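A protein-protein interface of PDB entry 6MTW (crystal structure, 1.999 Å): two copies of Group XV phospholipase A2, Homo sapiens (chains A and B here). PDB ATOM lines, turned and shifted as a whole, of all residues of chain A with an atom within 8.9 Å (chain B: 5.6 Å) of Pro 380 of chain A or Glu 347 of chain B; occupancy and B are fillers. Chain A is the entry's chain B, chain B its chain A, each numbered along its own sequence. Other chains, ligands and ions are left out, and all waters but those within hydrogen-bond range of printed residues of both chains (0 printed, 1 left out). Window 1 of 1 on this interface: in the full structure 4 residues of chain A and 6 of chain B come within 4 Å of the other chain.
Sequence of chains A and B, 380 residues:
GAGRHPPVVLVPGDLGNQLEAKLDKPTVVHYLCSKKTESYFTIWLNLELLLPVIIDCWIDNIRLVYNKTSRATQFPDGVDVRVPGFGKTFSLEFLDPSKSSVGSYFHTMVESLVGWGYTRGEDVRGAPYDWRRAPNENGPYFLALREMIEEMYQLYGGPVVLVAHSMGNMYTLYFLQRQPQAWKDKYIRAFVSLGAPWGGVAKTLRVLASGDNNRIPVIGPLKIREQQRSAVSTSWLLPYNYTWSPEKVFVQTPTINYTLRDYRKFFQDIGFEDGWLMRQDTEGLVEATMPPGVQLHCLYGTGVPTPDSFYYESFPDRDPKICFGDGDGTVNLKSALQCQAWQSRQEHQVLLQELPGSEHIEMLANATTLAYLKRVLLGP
Hydrophobic or aromatic side chains of chain B within 4 Å of the printed part of chain A: His 348.
Hydrophobic or aromatic side chains of chain A that line the printed part of chain B: Pro 380.
Among the printed residues, 13 pairs touch across the chains.
Among the printed residues, no Asp or Glu carboxylate lies within 4 Å of a Lys or Arg side-chain nitrogen of the other chain.
No position is printed for both chains.
Of the 13 pairs that touch across the chains among the printed residues, none has its exchanged pair printed and touching as well.
Glu 347 of chain B touches Arg 375 of chain A (CG to NH2, 3.97 Å).
Leu 378 of chain A touches Arg 345 of chain B.
Gly 379 of chain A touches Arg 345 of chain B (CA to O, 3.6 Å).
Gly 379 of chain A touches Gln 346 of chain B.
OE1 of Gln 181 of chain B touches CB of Pro 380 of chain A (3.3 Å).
Pro 380 of chain A touches Gly 293 of chain B (CG to CA, 3.8 Å).
Arg 345 of chain B touches Pro 380 of chain A.
CG of Pro 380 of chain A touches CB of Gln 346 of chain B (3.6 Å).
Printed residues of chain B within 4 Å of Pro 380 of chain A: Gln 181 (3.3 Å), Gly 293 (3.8 Å), Arg 345 (3.4 Å), Gln 346 (3.6 Å), Glu 347 (3.3 Å) and His 348 (2.5 Å).
Of chain A, only Arg 375, Leu 378, Gly 379 and Pro 380 come within 4 Å of Glu 347 of chain B.
Printed residues of chain A within 4 Å of Arg 345 of chain B: Leu 378, Gly 379 and Pro 380.
Of the printed residues of chain A, Gln 346 of chain B touches Leu 378 (3.0 Å), Gly 379 (3.96 Å) and Pro 380 (3.6 Å).
Of the printed residues of chain B, Leu 378 of chain A touches Arg 345, Gln 346 and Glu 347.
Gln 349 of chain B touches none of the printed residues of chain A.
Pro 291 of chain B touches none of the printed residues of chain A.
The nearest printed residue of chain A that does not touch Gln 346 of chain B is Leu 377 of chain A (7.0 Å).
The side-chain amide nitrogen of Gln 181 of chain B lies within hydrogen-bond range of the side-chain carboxylate of Asp 185 of chain B.
A ring nitrogen (ND1) of His 348 of chain B sits at hydrogen-bond distance from the backbone carbonyl oxygen (O) of Gly 293 of chain B.
OE1 of Gln 346 of chain B lies within hydrogen-bond range of N of Gly 293 of chain B (3.0 Å).
O of Val 294 of chain B lies within hydrogen-bond range of NE2 of Gln 346 of chain B (2.8 Å).
O of His 348 of chain B is in hydrogen-bond range of NE2 of Gln 346 of chain B.
O of Gly 293 of chain B lies within hydrogen-bond range of NE2 of Gln 181 of chain B.
N of Glu 347 of chain B sits close to O of Gly 379 of chain A, at 3.5 Å.
The backbone carbonyl oxygen (O) of Pro 380 of chain A is in hydrogen-bond range of the backbone NH (N) of Glu 347 of chain B.
The backbone NH (N) of Glu 347 of chain B sits at hydrogen-bond distance from the backbone carbonyl oxygen (O) of Leu 378 of chain A.
O of Leu 378 of chain A sits close to O of Gln 346 of chain B (3.4 Å).
ND1 of His 348 of chain B sits at hydrogen-bond distance from O of Pro 380 of chain A (2.5 Å).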
ATOM      1  N   TRP A 116      20.225 -14.418 -18.785  1.00  0.00           N
ATOM      2  CA  TRP A 116      19.181 -14.060 -19.736  1.00  0.00           C
ATOM      3  C   TRP A 116      18.812 -15.206 -20.668  1.00  0.00           C
ATOM      4  O   TRP A 116      17.961 -15.022 -21.543  1.00  0.00           O
ATOM      5  CB  TRP A 116      19.619 -12.854 -20.567  1.00  0.00           C
ATOM      6  CG  TRP A 116      19.993 -11.653 -19.754  1.00  0.00           C
ATOM      7  CD1 TRP A 116      19.492 -11.291 -18.531  1.00  0.00           C
ATOM      8  CD2 TRP A 116      20.964 -10.662 -20.099  1.00  0.00           C
ATOM      9  NE1 TRP A 116      20.089 -10.126 -18.102  1.00  0.00           N
ATOM     10  CE2 TRP A 116      20.994  -9.719 -19.047  1.00  0.00           C
ATOM     11  CE3 TRP A 116      21.804 -10.472 -21.202  1.00  0.00           C
ATOM     12  CZ2 TRP A 116      21.836  -8.609 -19.067  1.00  0.00           C
ATOM     13  CZ3 TRP A 116      22.641  -9.368 -21.216  1.00  0.00           C
ATOM     14  CH2 TRP A 116      22.651  -8.454 -20.156  1.00  0.00           C
ATOM     15  N   ARG A 189      23.860  -8.901 -36.955  1.00  0.00           N
ATOM     16  CA  ARG A 189      22.716  -8.123 -36.491  1.00  0.00           C
ATOM     17  C   ARG A 189      23.146  -6.744 -36.003  1.00  0.00           C
ATOM     18  O   ARG A 189      22.553  -5.730 -36.384  1.00  0.00           O
ATOM     19  CB  ARG A 189      21.979  -8.876 -35.381  1.00  0.00           C
ATOM     20  CG  ARG A 189      20.926  -8.045 -34.662  1.00  0.00           C
ATOM     21  CD  ARG A 189      19.922  -8.933 -33.943  1.00  0.00           C
ATOM     22  NE  ARG A 189      18.920  -8.154 -33.219  1.00  0.00           N
ATOM     23  CZ  ARG A 189      17.945  -8.686 -32.488  1.00  0.00           C
ATOM     24  NH1 ARG A 189      17.835 -10.003 -32.383  1.00  0.00           N
ATOM     25  NH2 ARG A 189      17.078  -7.902 -31.860  1.00  0.00           N
ATOM     26  N   ALA A 371      23.070  -3.234 -18.742  1.00  0.00           N
ATOM     27  CA  ALA A 371      21.676  -2.879 -18.974  1.00  0.00           C
ATOM     28  C   ALA A 371      21.461  -2.416 -20.408  1.00  0.00           C
ATOM     29  O   ALA A 371      20.440  -2.746 -21.024  1.00  0.00           O
ATOM     30  CB  ALA A 371      21.231  -1.802 -17.985  1.00  0.00           C
ATOM     31  N   LYS A 374      21.551  -5.495 -22.578  1.00  0.00           N
ATOM     32  CA  LYS A 374      20.349  -6.312 -22.443  1.00  0.00           C
ATOM     33  C   LYS A 374      19.247  -5.847 -23.390  1.00  0.00           C
ATOM     34  O   LYS A 374      18.562  -6.671 -24.008  1.00  0.00           O
ATOM     35  CB  LYS A 374      19.865  -6.287 -20.995  1.00  0.00           C
ATOM     36  CG  LYS A 374      18.786  -7.300 -20.678  1.00  0.00           C
ATOM     37  CD  LYS A 374      18.373  -7.212 -19.208  1.00  0.00           C
ATOM     38  CE  LYS A 374      17.249  -8.186 -18.882  1.00  0.00           C
ATOM     39  NZ  LYS A 374      16.613  -7.878 -17.568  1.00  0.00           N
ATOM     40  N   ARG A 375      19.062  -4.532 -23.521  1.00  0.00           N
ATOM     41  CA  ARG A 375      18.049  -4.014 -24.440  1.00  0.00           C
ATOM     42  C   ARG A 375      18.400  -4.311 -25.894  1.00  0.00           C
ATOM     43  O   ARG A 375      17.502  -4.532 -26.713  1.00  0.00           O
ATOM     44  CB  ARG A 375      17.863  -2.512 -24.228  1.00  0.00           C
ATOM     45  CG  ARG A 375      17.796  -2.117 -22.761  1.00  0.00           C
ATOM     46  CD  ARG A 375      16.376  -2.155 -22.222  1.00  0.00           C
ATOM     47  NE  ARG A 375      16.363  -2.365 -20.776  1.00  0.00           N
ATOM     48  CZ  ARG A 375      16.210  -3.551 -20.193  1.00  0.00           C
ATOM     49  NH1 ARG A 375      16.218  -3.648 -18.870  1.00  0.00           N
ATOM     50  NH2 ARG A 375      16.042  -4.642 -20.929  1.00  0.00           N
ATOM     51  N   VAL A 376      19.690  -4.310 -26.233  1.00  0.00           N
ATOM     52  CA  VAL A 376      20.105  -4.617 -27.601  1.00  0.00           C
ATOM     53  C   VAL A 376      19.745  -6.054 -27.960  1.00  0.00           C
ATOM     54  O   VAL A 376      19.216  -6.331 -29.042  1.00  0.00           O
ATOM     55  CB  VAL A 376      21.613  -4.359 -27.771  1.00  0.00           C
ATOM     56  CG1 VAL A 376      22.089  -4.856 -29.128  1.00  0.00           C
ATOM     57  CG2 VAL A 376      21.922  -2.880 -27.594  1.00  0.00           C
ATOM     58  N   LEU A 377      20.022  -6.989 -27.050  1.00  0.00           N
ATOM     59  CA  LEU A 377      19.840  -8.406 -27.339  1.00  0.00           C
ATOM     60  C   LEU A 377      18.387  -8.837 -27.196  1.00  0.00           C
ATOM     61  O   LEU A 377      17.880  -9.597 -28.028  1.00  0.00           O
ATOM     62  CB  LEU A 377      20.719  -9.243 -26.411  1.00  0.00           C
ATOM     63  CG  LEU A 377      22.215  -8.940 -26.413  1.00  0.00           C
ATOM     64  CD1 LEU A 377      22.921  -9.853 -25.430  1.00  0.00           C
ATOM     65  CD2 LEU A 377      22.793  -9.093 -27.817  1.00  0.00           C
ATOM     66  N   LEU A 378      17.710  -8.384 -26.144  1.00  0.00           N
ATOM     67  CA  LEU A 378      16.368  -8.855 -25.835  1.00  0.00           C
ATOM     68  C   LEU A 378      15.269  -7.942 -26.360  1.00  0.00           C
ATOM     69  O   LEU A 378      14.106  -8.357 -26.390  1.00  0.00           O
ATOM     70  CB  LEU A 378      16.200  -9.009 -24.320  1.00  0.00           C
ATOM     71  CG  LEU A 378      17.165  -9.938 -23.580  1.00  0.00           C
ATOM     72  CD1 LEU A 378      16.539 -10.395 -22.266  1.00  0.00           C
ATOM     73  CD2 LEU A 378      17.578 -11.133 -24.433  1.00  0.00           C
ATOM     74  N   GLY A 379      15.602  -6.728 -26.785  1.00  0.00           N
ATOM     75  CA  GLY A 379      14.607  -5.791 -27.245  1.00  0.00           C
ATOM     76  C   GLY A 379      14.028  -4.999 -26.090  1.00  0.00           C
ATOM     77  O   GLY A 379      14.421  -5.176 -24.933  1.00  0.00           O
ATOM     78  N   PRO A 380      13.067  -4.107 -26.383  1.00  0.00           N
ATOM     79  CA  PRO A 380      12.456  -3.218 -25.384  1.00  0.00           C
ATOM     80  C   PRO A 380      11.844  -3.962 -24.200  1.00  0.00           C
ATOM     81  O   PRO A 380      10.634  -4.189 -24.181  1.00  0.00           O
ATOM     82  CB  PRO A 380      11.370  -2.483 -26.183  1.00  0.00           C
ATOM     83  CG  PRO A 380      11.118  -3.334 -27.380  1.00  0.00           C
ATOM     84  CD  PRO A 380      12.441  -3.954 -27.707  1.00  0.00           C
ATOM     85  N   GLN B 181      10.617   4.854 -26.804  1.00  0.00           N
ATOM     86  CA  GLN B 181      10.592   3.765 -25.834  1.00  0.00           C
ATOM     87  C   GLN B 181      10.561   4.297 -24.408  1.00  0.00           C
ATOM     88  O   GLN B 181       9.866   3.743 -23.545  1.00  0.00           O
ATOM     89  CB  GLN B 181      11.793   2.844 -26.043  1.00  0.00           C
ATOM     90  CG  GLN B 181      11.713   1.555 -25.244  1.00  0.00           C
ATOM     91  CD  GLN B 181      10.437   0.785 -25.530  1.00  0.00           C
ATOM     92  OE1 GLN B 181      10.118   0.503 -26.684  1.00  0.00           O
ATOM     93  NE2 GLN B 181       9.698   0.446 -24.479  1.00  0.00           N
ATOM     94  N   ASP B 185       7.902   3.252 -21.642  1.00  0.00           N
ATOM     95  CA  ASP B 185       8.390   2.651 -20.405  1.00  0.00           C
ATOM     96  C   ASP B 185       7.858   3.378 -19.177  1.00  0.00           C
ATOM     97  O   ASP B 185       7.657   2.757 -18.127  1.00  0.00           O
ATOM     98  CB  ASP B 185       9.919   2.637 -20.392  1.00  0.00           C
ATOM     99  CG  ASP B 185      10.507   1.591 -21.324  1.00  0.00           C
ATOM    100  OD1 ASP B 185       9.752   0.708 -21.787  1.00  0.00           O
ATOM    101  OD2 ASP B 185      11.726   1.651 -21.597  1.00  0.00           O
ATOM    102  N   PRO B 291       7.572  -4.749 -32.627  1.00  0.00           N
ATOM    103  CA  PRO B 291       6.648  -5.040 -31.524  1.00  0.00           C
ATOM    104  C   PRO B 291       6.161  -3.759 -30.874  1.00  0.00           C
ATOM    105  O   PRO B 291       6.725  -2.680 -31.112  1.00  0.00           O
ATOM    106  CB  PRO B 291       7.513  -5.862 -30.557  1.00  0.00           C
ATOM    107  CG  PRO B 291       8.893  -5.367 -30.800  1.00  0.00           C
ATOM    108  CD  PRO B 291       8.971  -5.048 -32.272  1.00  0.00           C
ATOM    109  N   GLY B 293       6.497  -2.933 -27.798  1.00  0.00           N
ATOM    110  CA  GLY B 293       7.458  -2.490 -26.807  1.00  0.00           C
ATOM    111  C   GLY B 293       6.900  -2.291 -25.417  1.00  0.00           C
ATOM    112  O   GLY B 293       7.507  -1.573 -24.618  1.00  0.00           O
ATOM    113  N   VAL B 294       5.752  -2.896 -25.107  1.00  0.00           N
ATOM    114  CA  VAL B 294       5.168  -2.890 -23.770  1.00  0.00           C
ATOM    115  C   VAL B 294       4.672  -4.300 -23.468  1.00  0.00           C
ATOM    116  O   VAL B 294       4.579  -5.151 -24.354  1.00  0.00           O
ATOM    117  CB  VAL B 294       4.012  -1.872 -23.635  1.00  0.00           C
ATOM    118  CG1 VAL B 294       4.476  -0.468 -23.995  1.00  0.00           C
ATOM    119  CG2 VAL B 294       2.845  -2.284 -24.514  1.00  0.00           C
ATOM    120  N   GLN B 343       7.522 -11.948 -29.321  1.00  0.00           N
ATOM    121  CA  GLN B 343       8.190 -12.391 -28.100  1.00  0.00           C
ATOM    122  C   GLN B 343       9.701 -12.233 -28.213  1.00  0.00           C
ATOM    123  O   GLN B 343      10.346 -11.654 -27.331  1.00  0.00           O
ATOM    124  CB  GLN B 343       7.822 -13.845 -27.798  1.00  0.00           C
ATOM    125  CG  GLN B 343       6.342 -14.072 -27.546  1.00  0.00           C
ATOM    126  CD  GLN B 343       6.011 -15.531 -27.287  1.00  0.00           C
ATOM    127  OE1 GLN B 343       6.825 -16.421 -27.536  1.00  0.00           O
ATOM    128  NE2 GLN B 343       4.809 -15.781 -26.781  1.00  0.00           N
ATOM    129  N   ARG B 345      11.302 -10.294 -30.027  1.00  0.00           N
ATOM    130  CA  ARG B 345      11.673  -8.960 -30.470  1.00  0.00           C
ATOM    131  C   ARG B 345      11.599  -7.910 -29.368  1.00  0.00           C
ATOM    132  O   ARG B 345      12.057  -6.784 -29.578  1.00  0.00           O
ATOM    133  CB  ARG B 345      10.779  -8.545 -31.645  1.00  0.00           C
ATOM    134  CG  ARG B 345      10.810  -9.543 -32.793  1.00  0.00           C
ATOM    135  CD  ARG B 345       9.873  -9.149 -33.918  1.00  0.00           C
ATOM    136  NE  ARG B 345       9.931 -10.101 -35.026  1.00  0.00           N
ATOM    137  CZ  ARG B 345       8.958 -10.272 -35.915  1.00  0.00           C
ATOM    138  NH1 ARG B 345       7.845  -9.563 -35.826  1.00  0.00           N
ATOM    139  NH2 ARG B 345       9.096 -11.161 -36.889  1.00  0.00           N
ATOM    140  N   GLN B 346      11.047  -8.245 -28.204  1.00  0.00           N
ATOM    141  CA  GLN B 346      10.943  -7.293 -27.109  1.00  0.00           C
ATOM    142  C   GLN B 346      11.184  -8.013 -25.792  1.00  0.00           C
ATOM    143  O   GLN B 346      10.949  -9.218 -25.670  1.00  0.00           O
ATOM    144  CB  GLN B 346       9.574  -6.593 -27.085  1.00  0.00           C
ATOM    145  CG  GLN B 346       8.419  -7.469 -26.631  1.00  0.00           C
ATOM    146  CD  GLN B 346       7.110  -6.703 -26.548  1.00  0.00           C
ATOM    147  OE1 GLN B 346       6.796  -5.888 -27.418  1.00  0.00           O
ATOM    148  NE2 GLN B 346       6.342  -6.954 -25.492  1.00  0.00           N
ATOM    149  N   GLU B 347      11.667  -7.258 -24.805  1.00  0.00           N
ATOM    150  CA  GLU B 347      11.915  -7.830 -23.486  1.00  0.00           C
ATOM    151  C   GLU B 347      10.616  -8.014 -22.711  1.00  0.00           C
ATOM    152  O   GLU B 347      10.435  -9.035 -22.042  1.00  0.00           O
ATOM    153  CB  GLU B 347      12.896  -6.952 -22.705  1.00  0.00           C
ATOM    154  CG  GLU B 347      13.368  -7.544 -21.377  1.00  0.00           C
ATOM    155  CD  GLU B 347      12.411  -7.284 -20.228  1.00  0.00           C
ATOM    156  OE1 GLU B 347      12.396  -8.094 -19.277  1.00  0.00           O
ATOM    157  OE2 GLU B 347      11.669  -6.279 -20.276  1.00  0.00           O
ATOM    158  N   HIS B 348       9.714  -7.034 -22.785  1.00  0.00           N
ATOM    159  CA  HIS B 348       8.463  -7.101 -22.040  1.00  0.00           C
ATOM    160  C   HIS B 348       7.687  -8.357 -22.417  1.00  0.00           C
ATOM    161  O   HIS B 348       7.725  -8.820 -23.561  1.00  0.00           O
ATOM    162  CB  HIS B 348       7.605  -5.867 -22.320  1.00  0.00           C
ATOM    163  CG  HIS B 348       8.128  -4.608 -21.702  1.00  0.00           C
ATOM    164  ND1 HIS B 348       8.934  -3.724 -22.386  1.00  0.00           N
ATOM    165  CD2 HIS B 348       7.954  -4.083 -20.466  1.00  0.00           C
ATOM    166  CE1 HIS B 348       9.236  -2.708 -21.597  1.00  0.00           C
ATOM    167  NE2 HIS B 348       8.653  -2.901 -20.427  1.00  0.00           N
ATOM    168  N   GLN B 349       6.967  -8.902 -21.438  1.00  0.00           N
ATOM    169  CA  GLN B 349       6.263 -10.159 -21.636  1.00  0.00           C
ATOM    170  C   GLN B 349       5.199 -10.020 -22.716  1.00  0.00           C
ATOM    171  O   GLN B 349       4.546  -8.980 -22.840  1.00  0.00           O
ATOM    172  CB  GLN B 349       5.615 -10.617 -20.329  1.00  0.00           C
ATOM    173  CG  GLN B 349       6.147 -11.938 -19.804  1.00  0.00           C
ATOM    174  CD  GLN B 349       5.308 -12.491 -18.668  1.00  0.00           C
ATOM    175  OE1 GLN B 349       4.494 -11.782 -18.079  1.00  0.00           O
ATOM    176  NE2 GLN B 349       5.504 -13.767 -18.356  1.00  0.00           N
